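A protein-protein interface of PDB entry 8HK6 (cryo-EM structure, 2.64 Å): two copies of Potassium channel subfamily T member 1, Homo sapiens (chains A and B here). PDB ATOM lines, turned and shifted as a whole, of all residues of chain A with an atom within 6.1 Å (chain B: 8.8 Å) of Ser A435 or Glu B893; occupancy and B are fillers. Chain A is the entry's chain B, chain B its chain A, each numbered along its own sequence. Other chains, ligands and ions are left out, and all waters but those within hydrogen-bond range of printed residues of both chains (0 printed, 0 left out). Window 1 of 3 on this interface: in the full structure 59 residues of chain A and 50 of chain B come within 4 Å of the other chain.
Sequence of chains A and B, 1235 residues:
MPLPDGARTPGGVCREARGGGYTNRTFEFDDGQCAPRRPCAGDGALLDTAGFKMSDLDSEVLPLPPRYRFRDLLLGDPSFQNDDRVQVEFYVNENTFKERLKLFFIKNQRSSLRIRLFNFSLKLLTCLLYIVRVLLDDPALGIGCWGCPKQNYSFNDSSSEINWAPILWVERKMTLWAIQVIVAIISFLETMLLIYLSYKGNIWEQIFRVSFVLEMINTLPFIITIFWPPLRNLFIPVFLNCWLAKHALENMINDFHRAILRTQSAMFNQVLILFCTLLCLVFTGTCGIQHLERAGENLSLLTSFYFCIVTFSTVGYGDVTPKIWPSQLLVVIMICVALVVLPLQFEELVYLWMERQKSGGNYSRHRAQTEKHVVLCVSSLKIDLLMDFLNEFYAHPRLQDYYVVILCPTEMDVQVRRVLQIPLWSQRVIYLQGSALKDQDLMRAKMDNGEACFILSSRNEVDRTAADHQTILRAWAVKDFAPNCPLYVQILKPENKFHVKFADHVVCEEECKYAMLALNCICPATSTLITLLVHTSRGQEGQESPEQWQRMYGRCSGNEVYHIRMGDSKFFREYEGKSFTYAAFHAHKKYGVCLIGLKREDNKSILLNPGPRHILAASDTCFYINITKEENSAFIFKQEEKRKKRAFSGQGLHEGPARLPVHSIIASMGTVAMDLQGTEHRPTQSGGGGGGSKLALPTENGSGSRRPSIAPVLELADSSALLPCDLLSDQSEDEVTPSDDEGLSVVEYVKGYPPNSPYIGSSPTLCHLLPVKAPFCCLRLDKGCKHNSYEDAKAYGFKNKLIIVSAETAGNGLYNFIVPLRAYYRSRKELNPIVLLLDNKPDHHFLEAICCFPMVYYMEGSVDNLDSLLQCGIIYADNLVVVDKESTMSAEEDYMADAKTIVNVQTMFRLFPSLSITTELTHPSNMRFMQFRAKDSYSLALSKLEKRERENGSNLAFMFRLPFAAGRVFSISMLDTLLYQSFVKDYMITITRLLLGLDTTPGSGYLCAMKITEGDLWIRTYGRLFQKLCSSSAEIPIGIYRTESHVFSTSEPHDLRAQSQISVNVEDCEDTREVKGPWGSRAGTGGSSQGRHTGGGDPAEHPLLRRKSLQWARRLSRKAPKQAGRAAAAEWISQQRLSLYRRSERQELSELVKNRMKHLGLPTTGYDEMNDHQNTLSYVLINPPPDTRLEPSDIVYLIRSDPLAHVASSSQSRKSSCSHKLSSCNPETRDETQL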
ATOM      1  N   CYS A 377       9.868   1.079  -7.509  1.00  0.00           N
ATOM      2  CA  CYS A 377       8.927   2.117  -7.911  1.00  0.00           C
ATOM      3  C   CYS A 377       9.695   3.393  -8.235  1.00  0.00           C
ATOM      4  O   CYS A 377      10.300   4.005  -7.351  1.00  0.00           O
ATOM      5  CB  CYS A 377       7.893   2.356  -6.814  1.00  0.00           C
ATOM      6  SG  CYS A 377       6.511   3.385  -7.312  1.00  0.00           S
ATOM      7  N   SER A 379       9.666   7.023 -11.130  1.00  0.00           N
ATOM      8  CA  SER A 379       8.843   7.834 -12.018  1.00  0.00           C
ATOM      9  C   SER A 379       9.300   7.727 -13.464  1.00  0.00           C
ATOM     10  O   SER A 379       8.473   7.745 -14.381  1.00  0.00           O
ATOM     11  CB  SER A 379       8.862   9.297 -11.577  1.00  0.00           C
ATOM     12  OG  SER A 379      10.151   9.851 -11.740  1.00  0.00           O
ATOM     13  N   LEU A 407       7.795  -0.823 -11.354  1.00  0.00           N
ATOM     14  CA  LEU A 407       6.506  -0.154 -11.486  1.00  0.00           C
ATOM     15  C   LEU A 407       6.772   1.306 -11.833  1.00  0.00           C
ATOM     16  O   LEU A 407       7.045   2.123 -10.952  1.00  0.00           O
ATOM     17  CB  LEU A 407       5.695  -0.293 -10.204  1.00  0.00           C
ATOM     18  CG  LEU A 407       4.256   0.216 -10.237  1.00  0.00           C
ATOM     19  CD1 LEU A 407       3.415  -0.604 -11.190  1.00  0.00           C
ATOM     20  CD2 LEU A 407       3.663   0.201  -8.847  1.00  0.00           C
ATOM     21  N   CYS A 408       6.693   1.636 -13.119  1.00  0.00           N
ATOM     22  CA  CYS A 408       6.973   2.977 -13.592  1.00  0.00           C
ATOM     23  C   CYS A 408       5.845   3.451 -14.495  1.00  0.00           C
ATOM     24  O   CYS A 408       5.478   2.748 -15.444  1.00  0.00           O
ATOM     25  CB  CYS A 408       8.302   3.034 -14.354  1.00  0.00           C
ATOM     26  SG  CYS A 408       8.706   4.648 -15.024  1.00  0.00           S
ATOM     27  N   PRO A 409       5.283   4.634 -14.232  1.00  0.00           N
ATOM     28  CA  PRO A 409       4.209   5.139 -15.105  1.00  0.00           C
ATOM     29  C   PRO A 409       4.655   5.390 -16.535  1.00  0.00           C
ATOM     30  O   PRO A 409       3.828   5.366 -17.454  1.00  0.00           O
ATOM     31  CB  PRO A 409       3.783   6.438 -14.408  1.00  0.00           C
ATOM     32  CG  PRO A 409       4.957   6.833 -13.587  1.00  0.00           C
ATOM     33  CD  PRO A 409       5.590   5.565 -13.136  1.00  0.00           C
ATOM     34  N   GLN A 433       4.041  -0.873 -16.385  1.00  0.00           N
ATOM     35  CA  GLN A 433       3.653   0.522 -16.541  1.00  0.00           C
ATOM     36  C   GLN A 433       2.440   0.772 -15.655  1.00  0.00           C
ATOM     37  O   GLN A 433       1.338   0.301 -15.950  1.00  0.00           O
ATOM     38  CB  GLN A 433       3.358   0.857 -17.998  1.00  0.00           C
ATOM     39  CG  GLN A 433       2.891   2.281 -18.191  1.00  0.00           C
ATOM     40  CD  GLN A 433       3.092   2.776 -19.601  1.00  0.00           C
ATOM     41  OE1 GLN A 433       3.795   2.156 -20.394  1.00  0.00           O
ATOM     42  NE2 GLN A 433       2.480   3.907 -19.921  1.00  0.00           N
ATOM     43  N   GLY A 434       2.645   1.505 -14.572  1.00  0.00           N
ATOM     44  CA  GLY A 434       1.564   1.775 -13.647  1.00  0.00           C
ATOM     45  C   GLY A 434       2.027   2.714 -12.560  1.00  0.00           C
ATOM     46  O   GLY A 434       3.162   3.198 -12.562  1.00  0.00           O
ATOM     47  N   SER A 435       1.122   2.967 -11.625  1.00  0.00           N
ATOM     48  CA  SER A 435       1.362   3.883 -10.524  1.00  0.00           C
ATOM     49  C   SER A 435       1.305   3.129  -9.207  1.00  0.00           C
ATOM     50  O   SER A 435       0.531   2.182  -9.054  1.00  0.00           O
ATOM     51  CB  SER A 435       0.330   5.014 -10.506  1.00  0.00           C
ATOM     52  OG  SER A 435       0.405   5.792 -11.684  1.00  0.00           O
ATOM     53  N   ALA A 436       2.132   3.554  -8.254  1.00  0.00           N
ATOM     54  CA  ALA A 436       1.946   3.085  -6.893  1.00  0.00           C
ATOM     55  C   ALA A 436       0.640   3.577  -6.299  1.00  0.00           C
ATOM     56  O   ALA A 436       0.189   3.029  -5.291  1.00  0.00           O
ATOM     57  CB  ALA A 436       3.116   3.526  -6.014  1.00  0.00           C
ATOM     58  N   LEU A 437       0.020   4.581  -6.907  1.00  0.00           N
ATOM     59  CA  LEU A 437      -1.181   5.208  -6.382  1.00  0.00           C
ATOM     60  C   LEU A 437      -2.453   4.557  -6.895  1.00  0.00           C
ATOM     61  O   LEU A 437      -3.547   4.966  -6.500  1.00  0.00           O
ATOM     62  CB  LEU A 437      -1.170   6.699  -6.720  1.00  0.00           C
ATOM     63  CG  LEU A 437      -0.593   7.573  -5.607  1.00  0.00           C
ATOM     64  CD1 LEU A 437       0.843   7.194  -5.320  1.00  0.00           C
ATOM     65  CD2 LEU A 437      -0.686   9.033  -5.971  1.00  0.00           C
ATOM     66  N   LYS A 438      -2.332   3.557  -7.761  1.00  0.00           N
ATOM     67  CA  LYS A 438      -3.443   2.714  -8.174  1.00  0.00           C
ATOM     68  C   LYS A 438      -3.243   1.341  -7.553  1.00  0.00           C
ATOM     69  O   LYS A 438      -2.252   0.665  -7.846  1.00  0.00           O
ATOM     70  CB  LYS A 438      -3.521   2.617  -9.696  1.00  0.00           C
ATOM     71  CG  LYS A 438      -4.444   3.632 -10.332  1.00  0.00           C
ATOM     72  CD  LYS A 438      -3.901   4.113 -11.662  1.00  0.00           C
ATOM     73  CE  LYS A 438      -4.366   5.529 -11.964  1.00  0.00           C
ATOM     74  NZ  LYS A 438      -3.276   6.533 -11.798  1.00  0.00           N
ATOM     75  N   ASP A 439      -4.175   0.934  -6.691  1.00  0.00           N
ATOM     76  CA  ASP A 439      -4.051  -0.358  -6.027  1.00  0.00           C
ATOM     77  C   ASP A 439      -4.129  -1.516  -7.010  1.00  0.00           C
ATOM     78  O   ASP A 439      -3.700  -2.626  -6.682  1.00  0.00           O
ATOM     79  CB  ASP A 439      -5.132  -0.501  -4.958  1.00  0.00           C
ATOM     80  CG  ASP A 439      -5.220   0.712  -4.059  1.00  0.00           C
ATOM     81  OD1 ASP A 439      -5.697   1.766  -4.530  1.00  0.00           O
ATOM     82  OD2 ASP A 439      -4.808   0.617  -2.884  1.00  0.00           O
ATOM     83  N   GLN A 440      -4.675  -1.282  -8.203  1.00  0.00           N
ATOM     84  CA  GLN A 440      -4.652  -2.301  -9.244  1.00  0.00           C
ATOM     85  C   GLN A 440      -3.238  -2.529  -9.758  1.00  0.00           C
ATOM     86  O   GLN A 440      -2.834  -3.672  -9.997  1.00  0.00           O
ATOM     87  CB  GLN A 440      -5.585  -1.905 -10.389  1.00  0.00           C
ATOM     88  CG  GLN A 440      -7.066  -1.893 -10.026  1.00  0.00           C
ATOM     89  CD  GLN A 440      -7.957  -1.426 -11.163  1.00  0.00           C
ATOM     90  OE1 GLN A 440      -7.519  -0.692 -12.051  1.00  0.00           O
ATOM     91  NE2 GLN A 440      -9.215  -1.848 -11.139  1.00  0.00           N
ATOM     92  N   ASP A 441      -2.472  -1.452  -9.936  1.00  0.00           N
ATOM     93  CA  ASP A 441      -1.086  -1.593 -10.365  1.00  0.00           C
ATOM     94  C   ASP A 441      -0.210  -2.152  -9.255  1.00  0.00           C
ATOM     95  O   ASP A 441       0.780  -2.832  -9.536  1.00  0.00           O
ATOM     96  CB  ASP A 441      -0.546  -0.248 -10.840  1.00  0.00           C
ATOM     97  CG  ASP A 441      -1.271   0.268 -12.060  1.00  0.00           C
ATOM     98  OD1 ASP A 441      -1.806  -0.558 -12.827  1.00  0.00           O
ATOM     99  OD2 ASP A 441      -1.313   1.500 -12.254  1.00  0.00           O
ATOM    100  N   LEU A 442      -0.539  -1.865  -7.995  1.00  0.00           N
ATOM    101  CA  LEU A 442       0.165  -2.501  -6.894  1.00  0.00           C
ATOM    102  C   LEU A 442      -0.200  -3.971  -6.788  1.00  0.00           C
ATOM    103  O   LEU A 442       0.586  -4.760  -6.255  1.00  0.00           O
ATOM    104  CB  LEU A 442      -0.153  -1.801  -5.573  1.00  0.00           C
ATOM    105  CG  LEU A 442       0.300  -0.356  -5.377  1.00  0.00           C
ATOM    106  CD1 LEU A 442      -0.023   0.131  -3.982  1.00  0.00           C
ATOM    107  CD2 LEU A 442       1.739  -0.162  -5.732  1.00  0.00           C
ATOM    108  N   GLN A 470       5.953  13.361  -4.766  1.00  0.00           N
ATOM    109  CA  GLN A 470       5.527  12.131  -5.418  1.00  0.00           C
ATOM    110  C   GLN A 470       6.018  10.897  -4.674  1.00  0.00           C
ATOM    111  O   GLN A 470       5.285   9.911  -4.544  1.00  0.00           O
ATOM    112  CB  GLN A 470       6.022  12.123  -6.859  1.00  0.00           C
ATOM    113  CG  GLN A 470       5.532  13.308  -7.652  1.00  0.00           C
ATOM    114  CD  GLN A 470       5.669  13.110  -9.136  1.00  0.00           C
ATOM    115  OE1 GLN A 470       4.845  13.582  -9.913  1.00  0.00           O
ATOM    116  NE2 GLN A 470       6.715  12.406  -9.542  1.00  0.00           N
ATOM    117  N   ARG A 474       4.056   7.992  -2.976  1.00  0.00           N
ATOM    118  CA  ARG A 474       4.345   6.605  -3.314  1.00  0.00           C
ATOM    119  C   ARG A 474       4.650   5.782  -2.074  1.00  0.00           C
ATOM    120  O   ARG A 474       4.230   4.627  -1.971  1.00  0.00           O
ATOM    121  CB  ARG A 474       5.512   6.542  -4.289  1.00  0.00           C
ATOM    122  CG  ARG A 474       5.123   6.666  -5.727  1.00  0.00           C
ATOM    123  CD  ARG A 474       6.338   6.911  -6.579  1.00  0.00           C
ATOM    124  NE  ARG A 474       5.957   7.391  -7.897  1.00  0.00           N
ATOM    125  CZ  ARG A 474       6.663   8.250  -8.614  1.00  0.00           C
ATOM    126  NH1 ARG A 474       7.807   8.740  -8.173  1.00  0.00           N
ATOM    127  NH2 ARG A 474       6.207   8.627  -9.804  1.00  0.00           N
ATOM    128  N   LYS B 382     -10.805  10.793 -19.168  1.00  0.00           N
ATOM    129  CA  LYS B 382      -9.877   9.994 -18.393  1.00  0.00           C
ATOM    130  C   LYS B 382     -10.642   8.909 -17.654  1.00  0.00           C
ATOM    131  O   LYS B 382     -11.869   8.939 -17.551  1.00  0.00           O
ATOM    132  CB  LYS B 382      -9.077  10.867 -17.423  1.00  0.00           C
ATOM    133  CG  LYS B 382      -8.176  11.853 -18.134  1.00  0.00           C
ATOM    134  CD  LYS B 382      -7.063  12.344 -17.242  1.00  0.00           C
ATOM    135  CE  LYS B 382      -5.870  12.770 -18.073  1.00  0.00           C
ATOM    136  NZ  LYS B 382      -5.809  12.021 -19.358  1.00  0.00           N
ATOM    137  N   ASP B 384     -10.979   8.119 -14.629  1.00  0.00           N
ATOM    138  CA  ASP B 384     -11.712   8.454 -13.415  1.00  0.00           C
ATOM    139  C   ASP B 384     -13.063   9.067 -13.747  1.00  0.00           C
ATOM    140  O   ASP B 384     -14.071   8.765 -13.098  1.00  0.00           O
ATOM    141  CB  ASP B 384     -10.883   9.406 -12.561  1.00  0.00           C
ATOM    142  CG  ASP B 384      -9.417   9.069 -12.594  1.00  0.00           C
ATOM    143  OD1 ASP B 384      -8.735   9.458 -13.567  1.00  0.00           O
ATOM    144  OD2 ASP B 384      -8.957   8.383 -11.663  1.00  0.00           O
ATOM    145  N   GLN B 415      -5.552   4.006 -20.789  1.00  0.00           N
ATOM    146  CA  GLN B 415      -6.304   3.440 -19.675  1.00  0.00           C
ATOM    147  C   GLN B 415      -7.778   3.293 -20.025  1.00  0.00           C
ATOM    148  O   GLN B 415      -8.450   2.374 -19.548  1.00  0.00           O
ATOM    149  CB  GLN B 415      -6.134   4.315 -18.434  1.00  0.00           C
ATOM    150  CG  GLN B 415      -5.157   3.770 -17.415  1.00  0.00           C
ATOM    151  CD  GLN B 415      -4.653   4.839 -16.466  1.00  0.00           C
ATOM    152  OE1 GLN B 415      -4.986   4.843 -15.281  1.00  0.00           O
ATOM    153  NE2 GLN B 415      -3.843   5.754 -16.985  1.00  0.00           N
ATOM    154  N   ALA B 891      -0.075  17.438 -13.867  1.00  0.00           N
ATOM    155  CA  ALA B 891       0.695  16.207 -13.729  1.00  0.00           C
ATOM    156  C   ALA B 891       0.297  15.190 -14.791  1.00  0.00           C
ATOM    157  O   ALA B 891      -0.873  15.088 -15.159  1.00  0.00           O
ATOM    158  CB  ALA B 891       0.510  15.618 -12.341  1.00  0.00           C
ATOM    159  N   GLU B 892       1.280  14.438 -15.283  1.00  0.00           N
ATOM    160  CA  GLU B 892       1.005  13.402 -16.271  1.00  0.00           C
ATOM    161  C   GLU B 892       0.338  12.195 -15.622  1.00  0.00           C
ATOM    162  O   GLU B 892      -0.743  11.767 -16.041  1.00  0.00           O
ATOM    163  CB  GLU B 892       2.302  13.001 -16.976  1.00  0.00           C
ATOM    164  CG  GLU B 892       2.894  14.119 -17.817  1.00  0.00           C
ATOM    165  CD  GLU B 892       4.229  13.750 -18.427  1.00  0.00           C
ATOM    166  OE1 GLU B 892       4.788  12.700 -18.047  1.00  0.00           O
ATOM    167  OE2 GLU B 892       4.723  14.514 -19.284  1.00  0.00           O
ATOM    168  N   GLU B 893       0.970  11.634 -14.593  1.00  0.00           N
ATOM    169  CA  GLU B 893       0.297  10.658 -13.746  1.00  0.00           C
ATOM    170  C   GLU B 893      -0.805  11.359 -12.962  1.00  0.00           C
ATOM    171  O   GLU B 893      -0.547  12.328 -12.241  1.00  0.00           O
ATOM    172  CB  GLU B 893       1.305   9.998 -12.812  1.00  0.00           C
ATOM    173  CG  GLU B 893       0.695   9.274 -11.632  1.00  0.00           C
ATOM    174  CD  GLU B 893       1.741   8.574 -10.788  1.00  0.00           C
ATOM    175  OE1 GLU B 893       2.936   8.656 -11.134  1.00  0.00           O
ATOM    176  OE2 GLU B 893       1.370   7.942  -9.780  1.00  0.00           O
ATOM    177  N   ASP B 894      -2.035  10.870 -13.113  1.00  0.00           N
ATOM    178  CA  ASP B 894      -3.208  11.648 -12.727  1.00  0.00           C
ATOM    179  C   ASP B 894      -3.277  11.865 -11.221  1.00  0.00           C
ATOM    180  O   ASP B 894      -3.456  12.994 -10.752  1.00  0.00           O
ATOM    181  CB  ASP B 894      -4.474  10.955 -13.232  1.00  0.00           C
ATOM    182  CG  ASP B 894      -4.586  10.980 -14.743  1.00  0.00           C
ATOM    183  OD1 ASP B 894      -4.306  12.039 -15.342  1.00  0.00           O
ATOM    184  OD2 ASP B 894      -4.955   9.942 -15.333  1.00  0.00           O
ATOM    185  N   TYR B 895      -3.135  10.794 -10.442  1.00  0.00           N
ATOM    186  CA  TYR B 895      -3.340  10.891  -9.002  1.00  0.00           C
ATOM    187  C   TYR B 895      -2.292  11.757  -8.325  1.00  0.00           C
ATOM    188  O   TYR B 895      -2.482  12.157  -7.173  1.00  0.00           O
ATOM    189  CB  TYR B 895      -3.350   9.498  -8.378  1.00  0.00           C
ATOM    190  CG  TYR B 895      -4.582   8.685  -8.689  1.00  0.00           C
ATOM    191  CD1 TYR B 895      -5.541   9.153  -9.568  1.00  0.00           C
ATOM    192  CD2 TYR B 895      -4.782   7.449  -8.104  1.00  0.00           C
ATOM    193  CE1 TYR B 895      -6.660   8.415  -9.854  1.00  0.00           C
ATOM    194  CE2 TYR B 895      -5.904   6.702  -8.384  1.00  0.00           C
ATOM    195  CZ  TYR B 895      -6.841   7.192  -9.262  1.00  0.00           C
ATOM    196  OH  TYR B 895      -7.964   6.454  -9.551  1.00  0.00           O
ATOM    197  N   MET B 896      -1.195  12.063  -9.014  1.00  0.00           N
ATOM    198  CA  MET B 896      -0.153  12.904  -8.447  1.00  0.00           C
ATOM    199  C   MET B 896      -0.517  14.379  -8.461  1.00  0.00           C
ATOM    200  O   MET B 896       0.285  15.199  -8.006  1.00  0.00           O
ATOM    201  CB  MET B 896       1.156  12.679  -9.200  1.00  0.00           C
ATOM    202  CG  MET B 896       1.872  11.412  -8.793  1.00  0.00           C
ATOM    203  SD  MET B 896       2.324  11.408  -7.055  1.00  0.00           S
ATOM    204  CE  MET B 896       2.902   9.733  -6.870  1.00  0.00           C
ATOM    205  N   ALA B 897      -1.695  14.735  -8.976  1.00  0.00           N
ATOM    206  CA  ALA B 897      -2.104  16.133  -9.006  1.00  0.00           C
ATOM    207  C   ALA B 897      -2.353  16.677  -7.607  1.00  0.00           C
ATOM    208  O   ALA B 897      -2.189  17.878  -7.372  1.00  0.00           O
ATOM    209  CB  ALA B 897      -3.352  16.292  -9.870  1.00  0.00           C
ATOM    210  N   ASP B 898      -2.745  15.818  -6.671  1.00  0.00           N
ATOM    211  CA  ASP B 898      -2.987  16.226  -5.295  1.00  0.00           C
ATOM    212  C   ASP B 898      -1.746  16.149  -4.420  1.00  0.00           C
ATOM    213  O   ASP B 898      -1.839  16.436  -3.226  1.00  0.00           O
ATOM    214  CB  ASP B 898      -4.083  15.362  -4.666  1.00  0.00           C
ATOM    215  CG  ASP B 898      -5.352  15.336  -5.481  1.00  0.00           C
ATOM    216  OD1 ASP B 898      -5.851  16.417  -5.845  1.00  0.00           O
ATOM    217  OD2 ASP B 898      -5.862  14.232  -5.742  1.00  0.00           O
ATOM    218  N   ALA B 899      -0.594  15.774  -4.981  1.00  0.00           N
ATOM    219  CA  ALA B 899       0.568  15.466  -4.154  1.00  0.00           C
ATOM    220  C   ALA B 899       1.019  16.669  -3.338  1.00  0.00           C
ATOM    221  O   ALA B 899       1.331  16.538  -2.152  1.00  0.00           O
ATOM    222  CB  ALA B 899       1.710  14.952  -5.028  1.00  0.00           C
ATOM    223  N   HIS B 923      -9.167  13.727  -6.775  1.00  0.00           N
ATOM    224  CA  HIS B 923      -9.445  12.311  -6.885  1.00  0.00           C
ATOM    225  C   HIS B 923      -9.866  11.750  -5.536  1.00  0.00           C
ATOM    226  O   HIS B 923      -9.131  11.902  -4.552  1.00  0.00           O
ATOM    227  CB  HIS B 923      -8.215  11.559  -7.400  1.00  0.00           C
ATOM    228  CG  HIS B 923      -7.611  12.162  -8.629  1.00  0.00           C
ATOM    229  ND1 HIS B 923      -8.193  12.055  -9.873  1.00  0.00           N
ATOM    230  CD2 HIS B 923      -6.483  12.887  -8.803  1.00  0.00           C
ATOM    231  CE1 HIS B 923      -7.447  12.684 -10.761  1.00  0.00           C
ATOM    232  NE2 HIS B 923      -6.404  13.200 -10.137  1.00  0.00           N
ATOM    233  N   ASN B 926      -7.414   9.688  -3.448  1.00  0.00           N
ATOM    234  CA  ASN B 926      -6.388  10.339  -2.649  1.00  0.00           C
ATOM    235  C   ASN B 926      -6.880  10.742  -1.267  1.00  0.00           C
ATOM    236  O   ASN B 926      -6.091  11.270  -0.479  1.00  0.00           O
ATOM    237  CB  ASN B 926      -5.862  11.569  -3.391  1.00  0.00           C
ATOM    238  CG  ASN B 926      -5.063  11.208  -4.626  1.00  0.00           C
ATOM    239  OD1 ASN B 926      -4.567  10.095  -4.757  1.00  0.00           O
ATOM    240  ND2 ASN B 926      -4.944  12.151  -5.543  1.00  0.00           N
ATOM    241  N   ARG B 928      -7.449   8.989   1.231  1.00  0.00           N
ATOM    242  CA  ARG B 928      -6.807   8.219   2.290  1.00  0.00           C
ATOM    243  C   ARG B 928      -5.555   8.896   2.823  1.00  0.00           C
ATOM    244  O   ARG B 928      -5.111   8.568   3.929  1.00  0.00           O
ATOM    245  CB  ARG B 928      -6.451   6.828   1.781  1.00  0.00           C
ATOM    246  CG  ARG B 928      -6.296   6.771   0.292  1.00  0.00           C
ATOM    247  CD  ARG B 928      -5.448   5.613  -0.149  1.00  0.00           C
ATOM    248  NE  ARG B 928      -5.137   5.709  -1.568  1.00  0.00           N
ATOM    249  CZ  ARG B 928      -4.257   4.946  -2.199  1.00  0.00           C
ATOM    250  NH1 ARG B 928      -3.594   3.990  -1.572  1.00  0.00           N
ATOM    251  NH2 ARG B 928      -4.036   5.150  -3.493  1.00  0.00           N
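Hydrophobic or aromatic side chains of chain B that line the printed part of chain A: Tyr B895 and Met B896. Hydrophobic or aromatic side chains of chain A that line the printed part of chain B: Pro A409 and Leu A437. Among the printed residues, 11 pairs touch across the chains.
No residue of chain B comes within 4 Å of Gly A434. Ser A435 touches one residue of chain B. Glu B893 touches three residues of chain A. Printed residues of chain A within 4 Å of Tyr B895: Leu A437 (3.2 Å) and Lys A438 (3.9 Å). Of the printed residues of chain A, Met B896 touches Leu A437, Gln A470 and Arg A474. His B923 touches none of the printed residues of chain A. Asn B926 touches none of the printed residues of chain A. The nearest printed residue of chain A that does not touch Gln B415 is Asp A441 (5.8 Å).
The guanidinium group of Arg B928 is in hydrogen-bond range of the backbone carbonyl oxygen of Leu A437 (3.1 Å). The side-chain carboxylate of Glu B893 is in salt-bridge range of the guanidinium group of Arg A474 (3.5 Å). The side-chain hydroxyl (OG) of Ser A435 lies within hydrogen-bond range of the side-chain carboxylate (OE2) of Glu B893, 3.0 Å away. The guanidinium group (NH1) of Arg B928 is in salt-bridge range of the side-chain carboxylate (OD2) of Asp A439, at 3.8 Å.
NE2 of Gln A433 is in hydrogen-bond range of O of Pro A409. OD2 of Asp A441 is in hydrogen-bond range of N of Ser A435 (2.9 Å). OD2 of Asp B384 sits close to OH of Tyr B895 (3.0 Å). O of Tyr B895 is in hydrogen-bond range of ND2 of Asn B926, at 3.0 Å.
Pro A409 touches Glu B893 (CG to OE1, 3.7 Å). Tyr B895 touches Leu A437 (CD2 to O, 3.2 Å). CE of Met B896 touches CD1 of Leu A437 (3.6 Å). Lys A438 touches Gln B415. Lys A438 touches Tyr B895. O of Gln A470 touches CE of Met B896 (3.3 Å). Met B896 touches Arg A474 (CE to CG, 3.96 Å).
No position is printed for both chains. Of the 11 pairs that touch across the chains among the printed residues, none has its exchanged pair printed and touching as well.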
